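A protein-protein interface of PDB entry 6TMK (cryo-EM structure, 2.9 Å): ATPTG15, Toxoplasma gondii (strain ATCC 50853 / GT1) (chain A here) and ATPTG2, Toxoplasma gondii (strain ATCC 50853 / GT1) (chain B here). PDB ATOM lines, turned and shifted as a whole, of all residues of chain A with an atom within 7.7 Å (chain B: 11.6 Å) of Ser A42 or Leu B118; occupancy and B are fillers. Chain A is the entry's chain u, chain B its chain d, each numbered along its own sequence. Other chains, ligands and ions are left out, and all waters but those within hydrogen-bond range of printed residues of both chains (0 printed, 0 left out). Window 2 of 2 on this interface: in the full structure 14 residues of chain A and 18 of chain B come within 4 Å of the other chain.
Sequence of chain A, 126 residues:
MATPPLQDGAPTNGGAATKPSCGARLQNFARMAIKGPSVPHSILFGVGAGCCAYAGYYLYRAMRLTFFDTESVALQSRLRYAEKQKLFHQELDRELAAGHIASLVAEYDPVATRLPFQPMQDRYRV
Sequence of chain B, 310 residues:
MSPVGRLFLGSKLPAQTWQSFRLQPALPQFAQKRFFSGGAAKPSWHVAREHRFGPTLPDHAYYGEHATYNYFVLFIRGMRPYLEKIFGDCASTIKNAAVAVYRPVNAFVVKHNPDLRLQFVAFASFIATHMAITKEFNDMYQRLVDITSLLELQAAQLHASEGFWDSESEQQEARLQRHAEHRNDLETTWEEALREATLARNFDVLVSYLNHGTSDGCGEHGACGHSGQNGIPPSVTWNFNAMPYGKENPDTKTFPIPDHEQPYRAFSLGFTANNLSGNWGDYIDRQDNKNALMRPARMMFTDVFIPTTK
OD1 of Asn B113 lies within hydrogen-bond range of OG of Ser A42, 2.5 Å away. ND1 of His B112 sits at hydrogen-bond distance from NE2 of His A41, 3.1 Å away.
Ser A42 touches Leu B118 (OG to CB, 3.5 Å). Ala B122 touches Ser A42 (CA to O, 3.6 Å). Ile A43 touches Val B121. Ser B125 touches Ile A43 (OG to CA, 3.5 Å). Phe A45 touches Phe B108. CZ of Phe A45 touches CG2 of Val B109 (3.8 Å). Asn B113 touches Phe A45. Ala B122 touches Gly A46. Phe B126 touches Gly A46. Ala A49 touches Phe B126.
Of the 23 printed residues of chain B, 10 touch a printed residue of chain A. Hydrophobic or aromatic side chains of chain B that line the printed part of chain A: Phe B108, Val B109, His B112, Leu B118, Val B121, Ala B122 and Phe B126. Along chain A the printed residues that touch a printed residue of chain B span positions 41 to 49. Among the printed residues, 14 pairs touch across the chains.
O of Ser B125 lies within hydrogen-bond range of OG1 of Thr B129, 2.8 Å away. O of Val B121 lies within hydrogen-bond range of OG of Ser B125 (2.7 Å). OG of Ser A42 sits at hydrogen-bond distance from O of Ser A38, at 3.0 Å. The backbone carbonyl oxygen (O) of Asn B113 sits at hydrogen-bond distance from the side-chain amide nitrogen (NE2) of Gln B119, 3.1 Å away. OG of Ser A38 sits at hydrogen-bond distance from N of His A41 (3.3 Å).
No residue of chain B comes within 4 Å of Pro A37. No residue of chain B comes within 4 Å of Val A39. No residue of chain B comes within 4 Å of Pro A40. His A41 touches just one residue of chain B: His B112. Of chain B, only Asn B113, Leu B118, Val B121 and Ala B122 come within 4 Å of Ser A42. Ile A43 touches just these residues of chain B: Val B121 (3.8 Å) and Ser B125 (3.5 Å). Of the printed residues of chain B, Gly A46 touches Ala B122 (3.5 Å) and Phe B126 (3.4 Å). Of the printed residues of chain B, Val A47 touches Thr B129 (3.5 Å). Of the printed residues of chain B, Ala A49 touches Phe B126. Val B110 touches none of the printed residues of chain A. Leu B118 touches one residue of chain A. Printed residues of chain A within 4 Å of Val B121: Ser A42 and Ile A43. Ile B127 touches none of the printed residues of chain A. The nearest residue of chain B that does not touch Ser A42 is Ser B125 (4.4 Å). The nearest residue of chain A that does not touch Leu B118 is Val A39 (4.3 Å).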
ATOM      1  N   ALA A  33      30.086  27.099   6.491  1.00  0.00           N
ATOM      2  CA  ALA A  33      28.639  26.939   6.417  1.00  0.00           C
ATOM      3  C   ALA A  33      28.246  26.154   5.173  1.00  0.00           C
ATOM      4  O   ALA A  33      27.164  25.572   5.107  1.00  0.00           O
ATOM      5  CB  ALA A  33      27.960  28.295   6.418  1.00  0.00           C
ATOM      6  N   GLY A  36      31.530  22.397   5.827  1.00  0.00           N
ATOM      7  CA  GLY A  36      32.008  21.809   7.054  1.00  0.00           C
ATOM      8  C   GLY A  36      30.879  21.439   7.992  1.00  0.00           C
ATOM      9  O   GLY A  36      29.771  21.975   7.903  1.00  0.00           O
ATOM     10  N   PRO A  37      31.138  20.511   8.919  1.00  0.00           N
ATOM     11  CA  PRO A  37      30.117  20.175   9.919  1.00  0.00           C
ATOM     12  C   PRO A  37      29.915  21.294  10.922  1.00  0.00           C
ATOM     13  O   PRO A  37      30.769  21.548  11.777  1.00  0.00           O
ATOM     14  CB  PRO A  37      30.685  18.919  10.585  1.00  0.00           C
ATOM     15  CG  PRO A  37      32.150  19.067  10.448  1.00  0.00           C
ATOM     16  CD  PRO A  37      32.375  19.740   9.121  1.00  0.00           C
ATOM     17  N   SER A  38      28.775  21.967  10.820  1.00  0.00           N
ATOM     18  CA  SER A  38      28.521  23.175  11.586  1.00  0.00           C
ATOM     19  C   SER A  38      27.018  23.382  11.675  1.00  0.00           C
ATOM     20  O   SER A  38      26.236  22.724  10.985  1.00  0.00           O
ATOM     21  CB  SER A  38      29.216  24.384  10.955  1.00  0.00           C
ATOM     22  OG  SER A  38      28.672  24.686   9.684  1.00  0.00           O
ATOM     23  N   VAL A  39      26.622  24.308  12.547  1.00  0.00           N
ATOM     24  CA  VAL A  39      25.202  24.621  12.700  1.00  0.00           C
ATOM     25  C   VAL A  39      24.636  25.215  11.421  1.00  0.00           C
ATOM     26  O   VAL A  39      23.523  24.834  11.023  1.00  0.00           O
ATOM     27  CB  VAL A  39      24.989  25.515  13.928  1.00  0.00           C
ATOM     28  CG1 VAL A  39      23.630  26.168  13.881  1.00  0.00           C
ATOM     29  CG2 VAL A  39      25.143  24.707  15.191  1.00  0.00           C
ATOM     30  N   PRO A  40      25.302  26.152  10.745  1.00  0.00           N
ATOM     31  CA  PRO A  40      24.798  26.591   9.437  1.00  0.00           C
ATOM     32  C   PRO A  40      24.684  25.458   8.438  1.00  0.00           C
ATOM     33  O   PRO A  40      23.734  25.419   7.646  1.00  0.00           O
ATOM     34  CB  PRO A  40      25.842  27.623   8.999  1.00  0.00           C
ATOM     35  CG  PRO A  40      26.432  28.125  10.252  1.00  0.00           C
ATOM     36  CD  PRO A  40      26.424  26.979  11.211  1.00  0.00           C
ATOM     37  N   HIS A  41      25.639  24.530   8.453  1.00  0.00           N
ATOM     38  CA  HIS A  41      25.572  23.390   7.550  1.00  0.00           C
ATOM     39  C   HIS A  41      24.347  22.537   7.843  1.00  0.00           C
ATOM     40  O   HIS A  41      23.664  22.076   6.923  1.00  0.00           O
ATOM     41  CB  HIS A  41      26.849  22.567   7.672  1.00  0.00           C
ATOM     42  CG  HIS A  41      27.044  21.584   6.564  1.00  0.00           C
ATOM     43  ND1 HIS A  41      27.183  21.965   5.248  1.00  0.00           N
ATOM     44  CD2 HIS A  41      27.147  20.235   6.580  1.00  0.00           C
ATOM     45  CE1 HIS A  41      27.350  20.891   4.498  1.00  0.00           C
ATOM     46  NE2 HIS A  41      27.334  19.829   5.282  1.00  0.00           N
ATOM     47  N   SER A  42      24.044  22.331   9.124  1.00  0.00           N
ATOM     48  CA  SER A  42      22.865  21.555   9.486  1.00  0.00           C
ATOM     49  C   SER A  42      21.585  22.273   9.082  1.00  0.00           C
ATOM     50  O   SER A  42      20.616  21.639   8.648  1.00  0.00           O
ATOM     51  CB  SER A  42      22.876  21.278  10.985  1.00  0.00           C
ATOM     52  OG  SER A  42      24.086  20.662  11.375  1.00  0.00           O
ATOM     53  N   ILE A  43      21.556  23.597   9.231  1.00  0.00           N
ATOM     54  CA  ILE A  43      20.384  24.360   8.816  1.00  0.00           C
ATOM     55  C   ILE A  43      20.176  24.232   7.313  1.00  0.00           C
ATOM     56  O   ILE A  43      19.048  24.040   6.836  1.00  0.00           O
ATOM     57  CB  ILE A  43      20.529  25.826   9.252  1.00  0.00           C
ATOM     58  CG1 ILE A  43      20.451  25.926  10.771  1.00  0.00           C
ATOM     59  CG2 ILE A  43      19.450  26.673   8.632  1.00  0.00           C
ATOM     60  CD1 ILE A  43      21.063  27.168  11.325  1.00  0.00           C
ATOM     61  N   LEU A  44      21.258  24.350   6.545  1.00  0.00           N
ATOM     62  CA  LEU A  44      21.177  24.136   5.106  1.00  0.00           C
ATOM     63  C   LEU A  44      20.672  22.737   4.792  1.00  0.00           C
ATOM     64  O   LEU A  44      19.877  22.544   3.864  1.00  0.00           O
ATOM     65  CB  LEU A  44      22.545  24.362   4.473  1.00  0.00           C
ATOM     66  CG  LEU A  44      22.585  24.368   2.949  1.00  0.00           C
ATOM     67  CD1 LEU A  44      22.031  25.672   2.411  1.00  0.00           C
ATOM     68  CD2 LEU A  44      23.997  24.132   2.458  1.00  0.00           C
ATOM     69  N   PHE A  45      21.134  21.745   5.551  1.00  0.00           N
ATOM     70  CA  PHE A  45      20.690  20.374   5.338  1.00  0.00           C
ATOM     71  C   PHE A  45      19.190  20.247   5.543  1.00  0.00           C
ATOM     72  O   PHE A  45      18.495  19.598   4.751  1.00  0.00           O
ATOM     73  CB  PHE A  45      21.441  19.449   6.291  1.00  0.00           C
ATOM     74  CG  PHE A  45      21.347  18.004   5.932  1.00  0.00           C
ATOM     75  CD1 PHE A  45      22.235  17.440   5.041  1.00  0.00           C
ATOM     76  CD2 PHE A  45      20.372  17.205   6.492  1.00  0.00           C
ATOM     77  CE1 PHE A  45      22.150  16.110   4.715  1.00  0.00           C
ATOM     78  CE2 PHE A  45      20.282  15.877   6.168  1.00  0.00           C
ATOM     79  CZ  PHE A  45      21.170  15.328   5.279  1.00  0.00           C
ATOM     80  N   GLY A  46      18.669  20.866   6.601  1.00  0.00           N
ATOM     81  CA  GLY A  46      17.241  20.797   6.851  1.00  0.00           C
ATOM     82  C   GLY A  46      16.431  21.507   5.785  1.00  0.00           C
ATOM     83  O   GLY A  46      15.367  21.029   5.374  1.00  0.00           O
ATOM     84  N   VAL A  47      16.920  22.656   5.320  1.00  0.00           N
ATOM     85  CA  VAL A  47      16.238  23.357   4.237  1.00  0.00           C
ATOM     86  C   VAL A  47      16.198  22.490   2.986  1.00  0.00           C
ATOM     87  O   VAL A  47      15.165  22.388   2.308  1.00  0.00           O
ATOM     88  CB  VAL A  47      16.924  24.706   3.970  1.00  0.00           C
ATOM     89  CG1 VAL A  47      16.385  25.335   2.705  1.00  0.00           C
ATOM     90  CG2 VAL A  47      16.741  25.630   5.149  1.00  0.00           C
ATOM     91  N   GLY A  48      17.322  21.856   2.656  1.00  0.00           N
ATOM     92  CA  GLY A  48      17.343  20.980   1.501  1.00  0.00           C
ATOM     93  C   GLY A  48      16.395  19.810   1.652  1.00  0.00           C
ATOM     94  O   GLY A  48      15.748  19.392   0.689  1.00  0.00           O
ATOM     95  N   ALA A  49      16.303  19.262   2.863  1.00  0.00           N
ATOM     96  CA  ALA A  49      15.356  18.184   3.116  1.00  0.00           C
ATOM     97  C   ALA A  49      13.923  18.641   2.876  1.00  0.00           C
ATOM     98  O   ALA A  49      13.127  17.920   2.265  1.00  0.00           O
ATOM     99  CB  ALA A  49      15.520  17.673   4.543  1.00  0.00           C
ATOM    100  N   ASN B 106      20.837   7.132   6.138  1.00  0.00           N
ATOM    101  CA  ASN B 106      21.466   7.312   7.440  1.00  0.00           C
ATOM    102  C   ASN B 106      22.934   7.687   7.289  1.00  0.00           C
ATOM    103  O   ASN B 106      23.457   8.503   8.056  1.00  0.00           O
ATOM    104  CB  ASN B 106      21.314   6.038   8.267  1.00  0.00           C
ATOM    105  CG  ASN B 106      21.365   6.299   9.756  1.00  0.00           C
ATOM    106  OD1 ASN B 106      20.446   6.883  10.329  1.00  0.00           O
ATOM    107  ND2 ASN B 106      22.441   5.862  10.394  1.00  0.00           N
ATOM    108  N   PHE B 108      24.297   9.365   4.659  1.00  0.00           N
ATOM    109  CA  PHE B 108      24.331  10.742   4.183  1.00  0.00           C
ATOM    110  C   PHE B 108      23.980  11.727   5.286  1.00  0.00           C
ATOM    111  O   PHE B 108      24.486  12.853   5.297  1.00  0.00           O
ATOM    112  CB  PHE B 108      23.371  10.892   3.007  1.00  0.00           C
ATOM    113  CG  PHE B 108      23.379  12.252   2.385  1.00  0.00           C
ATOM    114  CD1 PHE B 108      24.515  12.742   1.774  1.00  0.00           C
ATOM    115  CD2 PHE B 108      22.240  13.034   2.392  1.00  0.00           C
ATOM    116  CE1 PHE B 108      24.520  13.989   1.196  1.00  0.00           C
ATOM    117  CE2 PHE B 108      22.241  14.282   1.813  1.00  0.00           C
ATOM    118  CZ  PHE B 108      23.382  14.760   1.217  1.00  0.00           C
ATOM    119  N   VAL B 109      23.122  11.325   6.220  1.00  0.00           N
ATOM    120  CA  VAL B 109      22.743  12.215   7.309  1.00  0.00           C
ATOM    121  C   VAL B 109      23.852  12.301   8.348  1.00  0.00           C
ATOM    122  O   VAL B 109      24.183  13.389   8.828  1.00  0.00           O
ATOM    123  CB  VAL B 109      21.418  11.745   7.930  1.00  0.00           C
ATOM    124  CG1 VAL B 109      21.214  12.371   9.291  1.00  0.00           C
ATOM    125  CG2 VAL B 109      20.268  12.082   7.017  1.00  0.00           C
ATOM    126  N   VAL B 110      24.441  11.162   8.716  1.00  0.00           N
ATOM    127  CA  VAL B 110      25.461  11.164   9.757  1.00  0.00           C
ATOM    128  C   VAL B 110      26.762  11.752   9.232  1.00  0.00           C
ATOM    129  O   VAL B 110      27.561  12.298  10.001  1.00  0.00           O
ATOM    130  CB  VAL B 110      25.664   9.739  10.296  1.00  0.00           C
ATOM    131  CG1 VAL B 110      26.866   9.690  11.209  1.00  0.00           C
ATOM    132  CG2 VAL B 110      24.422   9.277  11.024  1.00  0.00           C
ATOM    133  N   LYS B 111      27.000  11.648   7.925  1.00  0.00           N
ATOM    134  CA  LYS B 111      28.181  12.266   7.335  1.00  0.00           C
ATOM    135  C   LYS B 111      28.154  13.777   7.510  1.00  0.00           C
ATOM    136  O   LYS B 111      29.194  14.402   7.752  1.00  0.00           O
ATOM    137  CB  LYS B 111      28.262  11.902   5.854  1.00  0.00           C
ATOM    138  CG  LYS B 111      29.571  12.248   5.178  1.00  0.00           C
ATOM    139  CD  LYS B 111      30.680  11.306   5.596  1.00  0.00           C
ATOM    140  CE  LYS B 111      31.840  11.361   4.618  1.00  0.00           C
ATOM    141  NZ  LYS B 111      32.346  12.749   4.420  1.00  0.00           N
ATOM    142  N   HIS B 112      26.975  14.380   7.394  1.00  0.00           N
ATOM    143  CA  HIS B 112      26.814  15.824   7.463  1.00  0.00           C
ATOM    144  C   HIS B 112      26.326  16.314   8.818  1.00  0.00           C
ATOM    145  O   HIS B 112      26.397  17.518   9.083  1.00  0.00           O
ATOM    146  CB  HIS B 112      25.842  16.288   6.375  1.00  0.00           C
ATOM    147  CG  HIS B 112      26.329  16.038   4.983  1.00  0.00           C
ATOM    148  ND1 HIS B 112      26.604  17.055   4.096  1.00  0.00           N
ATOM    149  CD2 HIS B 112      26.597  14.886   4.327  1.00  0.00           C
ATOM    150  CE1 HIS B 112      27.015  16.540   2.952  1.00  0.00           C
ATOM    151  NE2 HIS B 112      27.020  15.225   3.066  1.00  0.00           N
ATOM    152  N   ASN B 113      25.835  15.424   9.677  1.00  0.00           N
ATOM    153  CA  ASN B 113      25.311  15.795  10.992  1.00  0.00           C
ATOM    154  C   ASN B 113      25.664  14.697  11.982  1.00  0.00           C
ATOM    155  O   ASN B 113      24.793  13.990  12.501  1.00  0.00           O
ATOM    156  CB  ASN B 113      23.800  16.019  10.926  1.00  0.00           C
ATOM    157  CG  ASN B 113      23.431  17.240  10.122  1.00  0.00           C
ATOM    158  OD1 ASN B 113      23.703  18.370  10.521  1.00  0.00           O
ATOM    159  ND2 ASN B 113      22.815  17.018   8.974  1.00  0.00           N
ATOM    160  N   PRO B 114      26.956  14.530  12.270  1.00  0.00           N
ATOM    161  CA  PRO B 114      27.394  13.378  13.071  1.00  0.00           C
ATOM    162  C   PRO B 114      26.926  13.402  14.515  1.00  0.00           C
ATOM    163  O   PRO B 114      26.880  12.339  15.144  1.00  0.00           O
ATOM    164  CB  PRO B 114      28.922  13.460  12.989  1.00  0.00           C
ATOM    165  CG  PRO B 114      29.200  14.893  12.722  1.00  0.00           C
ATOM    166  CD  PRO B 114      28.089  15.366  11.849  1.00  0.00           C
ATOM    167  N   ASP B 115      26.584  14.562  15.061  1.00  0.00           N
ATOM    168  CA  ASP B 115      26.273  14.700  16.475  1.00  0.00           C
ATOM    169  C   ASP B 115      24.785  14.940  16.692  1.00  0.00           C
ATOM    170  O   ASP B 115      24.049  15.340  15.786  1.00  0.00           O
ATOM    171  CB  ASP B 115      27.081  15.843  17.095  1.00  0.00           C
ATOM    172  CG  ASP B 115      27.258  15.683  18.590  1.00  0.00           C
ATOM    173  OD1 ASP B 115      28.109  14.869  19.003  1.00  0.00           O
ATOM    174  OD2 ASP B 115      26.545  16.368  19.351  1.00  0.00           O
ATOM    175  N   LEU B 116      24.356  14.686  17.930  1.00  0.00           N
ATOM    176  CA  LEU B 116      22.942  14.790  18.266  1.00  0.00           C
ATOM    177  C   LEU B 116      22.444  16.222  18.134  1.00  0.00           C
ATOM    178  O   LEU B 116      21.324  16.455  17.667  1.00  0.00           O
ATOM    179  CB  LEU B 116      22.706  14.280  19.684  1.00  0.00           C
ATOM    180  CG  LEU B 116      21.352  14.615  20.313  1.00  0.00           C
ATOM    181  CD1 LEU B 116      20.223  13.977  19.536  1.00  0.00           C
ATOM    182  CD2 LEU B 116      21.313  14.192  21.760  1.00  0.00           C
ATOM    183  N   ARG B 117      23.244  17.195  18.570  1.00  0.00           N
ATOM    184  CA  ARG B 117      22.794  18.580  18.503  1.00  0.00           C
ATOM    185  C   ARG B 117      22.616  19.015  17.055  1.00  0.00           C
ATOM    186  O   ARG B 117      21.661  19.727  16.721  1.00  0.00           O
ATOM    187  CB  ARG B 117      23.784  19.490  19.228  1.00  0.00           C
ATOM    188  CG  ARG B 117      25.199  19.412  18.707  1.00  0.00           C
ATOM    189  CD  ARG B 117      26.022  20.599  19.162  1.00  0.00           C
ATOM    190  NE  ARG B 117      26.344  20.541  20.580  1.00  0.00           N
ATOM    191  CZ  ARG B 117      27.136  21.411  21.194  1.00  0.00           C
ATOM    192  NH1 ARG B 117      27.381  21.287  22.486  1.00  0.00           N
ATOM    193  NH2 ARG B 117      27.679  22.410  20.516  1.00  0.00           N
ATOM    194  N   LEU B 118      23.499  18.552  16.172  1.00  0.00           N
ATOM    195  CA  LEU B 118      23.377  18.887  14.760  1.00  0.00           C
ATOM    196  C   LEU B 118      22.185  18.179  14.137  1.00  0.00           C
ATOM    197  O   LEU B 118      21.491  18.747  13.286  1.00  0.00           O
ATOM    198  CB  LEU B 118      24.662  18.521  14.029  1.00  0.00           C
ATOM    199  CG  LEU B 118      25.955  19.039  14.655  1.00  0.00           C
ATOM    200  CD1 LEU B 118      27.143  18.622  13.822  1.00  0.00           C
ATOM    201  CD2 LEU B 118      25.925  20.540  14.806  1.00  0.00           C
ATOM    202  N   GLN B 119      21.930  16.939  14.549  1.00  0.00           N
ATOM    203  CA  GLN B 119      20.745  16.236  14.074  1.00  0.00           C
ATOM    204  C   GLN B 119      19.477  16.969  14.485  1.00  0.00           C
ATOM    205  O   GLN B 119      18.544  17.115  13.687  1.00  0.00           O
ATOM    206  CB  GLN B 119      20.743  14.811  14.610  1.00  0.00           C
ATOM    207  CG  GLN B 119      21.681  13.886  13.877  1.00  0.00           C
ATOM    208  CD  GLN B 119      22.069  12.680  14.690  1.00  0.00           C
ATOM    209  OE1 GLN B 119      21.365  12.287  15.617  1.00  0.00           O
ATOM    210  NE2 GLN B 119      23.196  12.080  14.345  1.00  0.00           N
ATOM    211  N   PHE B 120      19.428  17.439  15.730  1.00  0.00           N
ATOM    212  CA  PHE B 120      18.263  18.173  16.206  1.00  0.00           C
ATOM    213  C   PHE B 120      18.101  19.483  15.448  1.00  0.00           C
ATOM    214  O   PHE B 120      16.982  19.869  15.088  1.00  0.00           O
ATOM    215  CB  PHE B 120      18.391  18.419  17.709  1.00  0.00           C
ATOM    216  CG  PHE B 120      17.334  19.319  18.273  1.00  0.00           C
ATOM    217  CD1 PHE B 120      16.004  18.940  18.268  1.00  0.00           C
ATOM    218  CD2 PHE B 120      17.675  20.540  18.822  1.00  0.00           C
ATOM    219  CE1 PHE B 120      15.035  19.771  18.791  1.00  0.00           C
ATOM    220  CE2 PHE B 120      16.710  21.372  19.345  1.00  0.00           C
ATOM    221  CZ  PHE B 120      15.391  20.988  19.332  1.00  0.00           C
ATOM    222  N   VAL B 121      19.211  20.171  15.179  1.00  0.00           N
ATOM    223  CA  VAL B 121      19.148  21.412  14.417  1.00  0.00           C
ATOM    224  C   VAL B 121      18.608  21.151  13.019  1.00  0.00           C
ATOM    225  O   VAL B 121      17.759  21.896  12.514  1.00  0.00           O
ATOM    226  CB  VAL B 121      20.539  22.068  14.370  1.00  0.00           C
ATOM    227  CG1 VAL B 121      20.598  23.113  13.286  1.00  0.00           C
ATOM    228  CG2 VAL B 121      20.879  22.673  15.703  1.00  0.00           C
ATOM    229  N   ALA B 122      19.098  20.097  12.367  1.00  0.00           N
ATOM    230  CA  ALA B 122      18.645  19.789  11.017  1.00  0.00           C
ATOM    231  C   ALA B 122      17.170  19.418  11.006  1.00  0.00           C
ATOM    232  O   ALA B 122      16.424  19.827  10.112  1.00  0.00           O
ATOM    233  CB  ALA B 122      19.486  18.661  10.432  1.00  0.00           C
ATOM    234  N   PHE B 123      16.732  18.648  12.001  1.00  0.00           N
ATOM    235  CA  PHE B 123      15.326  18.273  12.091  1.00  0.00           C
ATOM    236  C   PHE B 123      14.448  19.505  12.267  1.00  0.00           C
ATOM    237  O   PHE B 123      13.408  19.643  11.606  1.00  0.00           O
ATOM    238  CB  PHE B 123      15.129  17.291  13.241  1.00  0.00           C
ATOM    239  CG  PHE B 123      13.738  16.760  13.352  1.00  0.00           C
ATOM    240  CD1 PHE B 123      13.253  15.869  12.414  1.00  0.00           C
ATOM    241  CD2 PHE B 123      12.916  17.140  14.393  1.00  0.00           C
ATOM    242  CE1 PHE B 123      11.976  15.373  12.509  1.00  0.00           C
ATOM    243  CE2 PHE B 123      11.634  16.646  14.491  1.00  0.00           C
ATOM    244  CZ  PHE B 123      11.165  15.762  13.547  1.00  0.00           C
ATOM    245  N   ALA B 124      14.856  20.417  13.149  1.00  0.00           N
ATOM    246  CA  ALA B 124      14.069  21.620  13.384  1.00  0.00           C
ATOM    247  C   ALA B 124      14.027  22.504  12.144  1.00  0.00           C
ATOM    248  O   ALA B 124      12.985  23.089  11.826  1.00  0.00           O
ATOM    249  CB  ALA B 124      14.643  22.384  14.570  1.00  0.00           C
ATOM    250  N   SER B 125      15.148  22.620  11.432  1.00  0.00           N
ATOM    251  CA  SER B 125      15.164  23.417  10.212  1.00  0.00           C
ATOM    252  C   SER B 125      14.278  22.797   9.141  1.00  0.00           C
ATOM    253  O   SER B 125      13.588  23.512   8.404  1.00  0.00           O
ATOM    254  CB  SER B 125      16.596  23.560   9.710  1.00  0.00           C
ATOM    255  OG  SER B 125      17.459  23.952  10.759  1.00  0.00           O
ATOM    256  N   PHE B 126      14.287  21.469   9.039  1.00  0.00           N
ATOM    257  CA  PHE B 126      13.395  20.780   8.115  1.00  0.00           C
ATOM    258  C   PHE B 126      11.944  21.098   8.440  1.00  0.00           C
ATOM    259  O   PHE B 126      11.144  21.418   7.551  1.00  0.00           O
ATOM    260  CB  PHE B 126      13.669  19.278   8.186  1.00  0.00           C
ATOM    261  CG  PHE B 126      12.543  18.422   7.704  1.00  0.00           C
ATOM    262  CD1 PHE B 126      12.360  18.194   6.356  1.00  0.00           C
ATOM    263  CD2 PHE B 126      11.683  17.822   8.600  1.00  0.00           C
ATOM    264  CE1 PHE B 126      11.333  17.403   5.911  1.00  0.00           C
ATOM    265  CE2 PHE B 126      10.651  17.029   8.160  1.00  0.00           C
ATOM    266  CZ  PHE B 126      10.476  16.817   6.813  1.00  0.00           C
ATOM    267  N   ILE B 127      11.592  21.015   9.723  1.00  0.00           N
ATOM    268  CA  ILE B 127      10.227  21.311  10.146  1.00  0.00           C
ATOM    269  C   ILE B 127       9.854  22.739   9.772  1.00  0.00           C
ATOM    270  O   ILE B 127       8.766  22.999   9.245  1.00  0.00           O
ATOM    271  CB  ILE B 127      10.083  21.075  11.658  1.00  0.00           C
ATOM    272  CG1 ILE B 127      10.237  19.591  11.986  1.00  0.00           C
ATOM    273  CG2 ILE B 127       8.764  21.615  12.159  1.00  0.00           C
ATOM    274  CD1 ILE B 127       9.044  18.760  11.627  1.00  0.00           C
ATOM    275  N   ALA B 128      10.749  23.687  10.056  1.00  0.00           N
ATOM    276  CA  ALA B 128      10.450  25.087   9.783  1.00  0.00           C
ATOM    277  C   ALA B 128      10.268  25.339   8.294  1.00  0.00           C
ATOM    278  O   ALA B 128       9.370  26.084   7.889  1.00  0.00           O
ATOM    279  CB  ALA B 128      11.555  25.972  10.345  1.00  0.00           C
ATOM    280  N   THR B 129      11.110  24.729   7.459  1.00  0.00           N
ATOM    281  CA  THR B 129      10.990  24.922   6.019  1.00  0.00           C
ATOM    282  C   THR B 129       9.679  24.348   5.499  1.00  0.00           C
ATOM    283  O   THR B 129       8.983  24.980   4.687  1.00  0.00           O
ATOM    284  CB  THR B 129      12.177  24.275   5.311  1.00  0.00           C
ATOM    285  OG1 THR B 129      13.393  24.748   5.896  1.00  0.00           O
ATOM    286  CG2 THR B 129      12.169  24.611   3.839  1.00  0.00           C
